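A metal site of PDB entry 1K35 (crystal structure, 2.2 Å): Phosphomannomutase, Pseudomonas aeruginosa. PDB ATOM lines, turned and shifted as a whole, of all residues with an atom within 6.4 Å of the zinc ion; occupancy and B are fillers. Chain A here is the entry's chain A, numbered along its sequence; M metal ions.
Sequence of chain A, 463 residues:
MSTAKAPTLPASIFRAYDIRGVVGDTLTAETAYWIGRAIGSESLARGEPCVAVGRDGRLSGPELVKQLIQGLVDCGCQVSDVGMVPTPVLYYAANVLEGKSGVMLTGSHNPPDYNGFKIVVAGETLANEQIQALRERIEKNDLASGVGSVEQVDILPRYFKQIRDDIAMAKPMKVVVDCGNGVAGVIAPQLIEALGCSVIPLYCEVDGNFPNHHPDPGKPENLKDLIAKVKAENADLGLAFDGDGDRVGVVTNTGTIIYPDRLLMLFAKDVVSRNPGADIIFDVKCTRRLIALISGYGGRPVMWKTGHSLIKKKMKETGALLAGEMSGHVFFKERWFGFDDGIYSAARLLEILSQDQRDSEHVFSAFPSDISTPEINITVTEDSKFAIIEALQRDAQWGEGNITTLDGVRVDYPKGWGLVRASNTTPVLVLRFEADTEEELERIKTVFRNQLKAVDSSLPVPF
The backbone carbonyl oxygen (O) of Arg 247 sits at hydrogen-bond distance from the backbone NH (N) of Asp 242 (3.3 Å).
OD1 of Asp 242 sits at hydrogen-bond distance from N of Gly 245, at 2.9 Å.
O3P of SEP 108 sits close to the side-chain amino group (NZ) of Lys 118 (3.1 Å).
ND1 of His 109 sits at hydrogen-bond distance from O1P of SEP 108.
OG1 of Thr 106 is in hydrogen-bond range of N of SEP 108 (2.9 Å).
The side-chain amino group (NZ) of Lys 118 lies within salt-bridge range of the side-chain carboxylate (OD2) of Asp 246.
The side-chain carboxylate (OD2) of Asp 246 sits at hydrogen-bond distance from a ring nitrogen (NE2) of His 329, at 3.5 Å.
The side-chain carboxylate of Asp 244 lies within salt-bridge range of the side-chain amino group of Lys 118, at 3.2 Å.
NZ of Lys 118 touches the zinc ion, 3.6 Å away.
Of the 12 residues printed, 5 come within 4 Å of the zinc ion.
The zinc ion is bound by OD2 of Asp 242 (1.8 Å), O3P of SEP 108 (2.0 Å), OD1 of Asp 246 (2.0 Å) and OD2 of Asp 244 (2.2 Å).
Slightly farther from the zinc ion lies OG of SEP 108 (2.8 Å).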
ATOM      1  N   THR A  87     -21.692 -10.961  -6.340  1.00  0.00           N
ATOM      2  CA  THR A  87     -22.372 -10.806  -7.608  1.00  0.00           C
ATOM      3  C   THR A  87     -23.803 -10.303  -7.498  1.00  0.00           C
ATOM      4  O   THR A  87     -24.126  -9.340  -8.170  1.00  0.00           O
ATOM      5  CB  THR A  87     -22.311 -12.093  -8.356  1.00  0.00           C
ATOM      6  OG1 THR A  87     -21.009 -12.208  -8.961  1.00  0.00           O
ATOM      7  CG2 THR A  87     -23.334 -12.155  -9.505  1.00  0.00           C
ATOM      8  N   THR A 106     -15.445 -10.973 -11.924  1.00  0.00           N
ATOM      9  CA  THR A 106     -15.459 -12.258 -11.187  1.00  0.00           C
ATOM     10  C   THR A 106     -15.113 -13.478 -11.981  1.00  0.00           C
ATOM     11  O   THR A 106     -15.352 -13.555 -13.164  1.00  0.00           O
ATOM     12  CB  THR A 106     -16.837 -12.554 -10.534  1.00  0.00           C
ATOM     13  OG1 THR A 106     -16.768 -13.813  -9.833  1.00  0.00           O
ATOM     14  CG2 THR A 106     -17.916 -12.813 -11.583  1.00  0.00           C
ATOM     15  N   SEP A 108     -16.216 -16.526 -10.632  1.00  0.00           N
ATOM     16  CA  SEP A 108     -17.162 -17.506 -10.066  1.00  0.00           C
ATOM     17  CB  SEP A 108     -17.949 -18.226 -11.181  1.00  0.00           C
ATOM     18  OG  SEP A 108     -19.111 -18.914 -10.677  1.00  0.00           O
ATOM     19  C   SEP A 108     -16.487 -18.519  -9.157  1.00  0.00           C
ATOM     20  O   SEP A 108     -15.942 -18.176  -8.128  1.00  0.00           O
ATOM     21  P   SEP A 108     -20.373 -19.072 -11.727  1.00  0.00           P
ATOM     22  O1P SEP A 108     -20.272 -20.536 -12.354  1.00  0.00           O
ATOM     23  O2P SEP A 108     -20.301 -17.956 -12.858  1.00  0.00           O
ATOM     24  O3P SEP A 108     -21.791 -18.823 -11.022  1.00  0.00           O
ATOM     25  N   HIS A 109     -16.534 -19.789  -9.539  1.00  0.00           N
ATOM     26  CA  HIS A 109     -16.000 -20.839  -8.675  1.00  0.00           C
ATOM     27  C   HIS A 109     -14.726 -21.418  -9.233  1.00  0.00           C
ATOM     28  O   HIS A 109     -14.163 -22.347  -8.671  1.00  0.00           O
ATOM     29  CB  HIS A 109     -17.003 -21.971  -8.589  1.00  0.00           C
ATOM     30  CG  HIS A 109     -17.134 -22.712  -9.878  1.00  0.00           C
ATOM     31  ND1 HIS A 109     -17.707 -22.150 -10.994  1.00  0.00           N
ATOM     32  CD2 HIS A 109     -16.704 -23.942 -10.248  1.00  0.00           C
ATOM     33  CE1 HIS A 109     -17.655 -23.010 -11.997  1.00  0.00           C
ATOM     34  NE2 HIS A 109     -17.039 -24.102 -11.570  1.00  0.00           N
ATOM     35  N   LYS A 118     -19.269 -10.437 -15.602  1.00  0.00           N
ATOM     36  CA  LYS A 118     -20.671 -10.696 -15.819  1.00  0.00           C
ATOM     37  C   LYS A 118     -21.205  -9.311 -16.078  1.00  0.00           C
ATOM     38  O   LYS A 118     -20.963  -8.414 -15.247  1.00  0.00           O
ATOM     39  CB  LYS A 118     -21.301 -11.368 -14.595  1.00  0.00           C
ATOM     40  CG  LYS A 118     -20.843 -12.805 -14.440  1.00  0.00           C
ATOM     41  CD  LYS A 118     -21.446 -13.529 -13.239  1.00  0.00           C
ATOM     42  CE  LYS A 118     -20.750 -14.886 -13.100  1.00  0.00           C
ATOM     43  NZ  LYS A 118     -21.352 -15.920 -12.155  1.00  0.00           N
ATOM     44  N   ASP A 242     -21.168 -20.525  -3.650  1.00  0.00           N
ATOM     45  CA  ASP A 242     -20.087 -20.531  -4.601  1.00  0.00           C
ATOM     46  C   ASP A 242     -19.244 -19.226  -4.402  1.00  0.00           C
ATOM     47  O   ASP A 242     -19.560 -18.373  -3.549  1.00  0.00           O
ATOM     48  CB  ASP A 242     -20.598 -20.712  -6.045  1.00  0.00           C
ATOM     49  CG  ASP A 242     -21.103 -19.447  -6.662  1.00  0.00           C
ATOM     50  OD1 ASP A 242     -21.643 -18.645  -5.889  1.00  0.00           O
ATOM     51  OD2 ASP A 242     -21.044 -19.190  -7.915  1.00  0.00           O
ATOM     52  N   GLY A 243     -18.182 -19.099  -5.179  1.00  0.00           N
ATOM     53  CA  GLY A 243     -17.214 -18.004  -5.042  1.00  0.00           C
ATOM     54  C   GLY A 243     -17.740 -16.589  -4.972  1.00  0.00           C
ATOM     55  O   GLY A 243     -17.315 -15.762  -4.142  1.00  0.00           O
ATOM     56  N   ASP A 244     -18.687 -16.304  -5.844  1.00  0.00           N
ATOM     57  CA  ASP A 244     -19.186 -14.968  -6.010  1.00  0.00           C
ATOM     58  C   ASP A 244     -20.608 -14.815  -5.487  1.00  0.00           C
ATOM     59  O   ASP A 244     -21.214 -13.752  -5.610  1.00  0.00           O
ATOM     60  CB  ASP A 244     -19.115 -14.640  -7.480  1.00  0.00           C
ATOM     61  CG  ASP A 244     -19.993 -15.562  -8.274  1.00  0.00           C
ATOM     62  OD1 ASP A 244     -20.783 -15.104  -9.147  1.00  0.00           O
ATOM     63  OD2 ASP A 244     -19.959 -16.767  -8.003  1.00  0.00           O
ATOM     64  N   GLY A 245     -21.156 -15.903  -4.951  1.00  0.00           N
ATOM     65  CA  GLY A 245     -22.444 -15.840  -4.261  1.00  0.00           C
ATOM     66  C   GLY A 245     -23.759 -15.823  -5.002  1.00  0.00           C
ATOM     67  O   GLY A 245     -24.753 -15.467  -4.390  1.00  0.00           O
ATOM     68  N   ASP A 246     -23.793 -16.168  -6.277  1.00  0.00           N
ATOM     69  CA  ASP A 246     -25.077 -16.229  -7.002  1.00  0.00           C
ATOM     70  C   ASP A 246     -25.640 -17.634  -7.017  1.00  0.00           C
ATOM     71  O   ASP A 246     -26.695 -17.865  -7.644  1.00  0.00           O
ATOM     72  CB  ASP A 246     -24.996 -15.723  -8.462  1.00  0.00           C
ATOM     73  CG  ASP A 246     -23.868 -16.360  -9.249  1.00  0.00           C
ATOM     74  OD1 ASP A 246     -23.211 -17.280  -8.733  1.00  0.00           O
ATOM     75  OD2 ASP A 246     -23.559 -15.954 -10.413  1.00  0.00           O
ATOM     76  N   ARG A 247     -24.943 -18.548  -6.349  1.00  0.00           N
ATOM     77  CA  ARG A 247     -25.289 -19.956  -6.223  1.00  0.00           C
ATOM     78  C   ARG A 247     -25.281 -20.382  -4.740  1.00  0.00           C
ATOM     79  O   ARG A 247     -24.406 -19.978  -3.972  1.00  0.00           O
ATOM     80  CB  ARG A 247     -24.208 -20.746  -6.974  1.00  0.00           C
ATOM     81  CG  ARG A 247     -24.645 -21.975  -7.667  1.00  0.00           C
ATOM     82  CD  ARG A 247     -24.079 -22.094  -9.117  1.00  0.00           C
ATOM     83  NE  ARG A 247     -22.626 -22.209  -9.144  1.00  0.00           N
ATOM     84  CZ  ARG A 247     -21.947 -23.299  -8.815  1.00  0.00           C
ATOM     85  NH1 ARG A 247     -22.576 -24.403  -8.421  1.00  0.00           N
ATOM     86  NH2 ARG A 247     -20.616 -23.282  -8.873  1.00  0.00           N
ATOM     87  N   HIS A 329     -28.538 -21.852  -9.372  1.00  0.00           N
ATOM     88  CA  HIS A 329     -28.975 -20.486  -9.381  1.00  0.00           C
ATOM     89  C   HIS A 329     -30.478 -20.505  -9.127  1.00  0.00           C
ATOM     90  O   HIS A 329     -31.217 -21.200  -9.827  1.00  0.00           O
ATOM     91  CB  HIS A 329     -28.700 -19.880 -10.725  1.00  0.00           C
ATOM     92  CG  HIS A 329     -27.258 -19.655 -10.988  1.00  0.00           C
ATOM     93  ND1 HIS A 329     -26.447 -20.632 -11.512  1.00  0.00           N
ATOM     94  CD2 HIS A 329     -26.495 -18.558 -10.841  1.00  0.00           C
ATOM     95  CE1 HIS A 329     -25.235 -20.138 -11.661  1.00  0.00           C
ATOM     96  NE2 HIS A 329     -25.230 -18.882 -11.254  1.00  0.00           N
HETATM   97 ZN    ZN M   1     -21.370 -18.006  -9.217  1.00  0.00          ZN
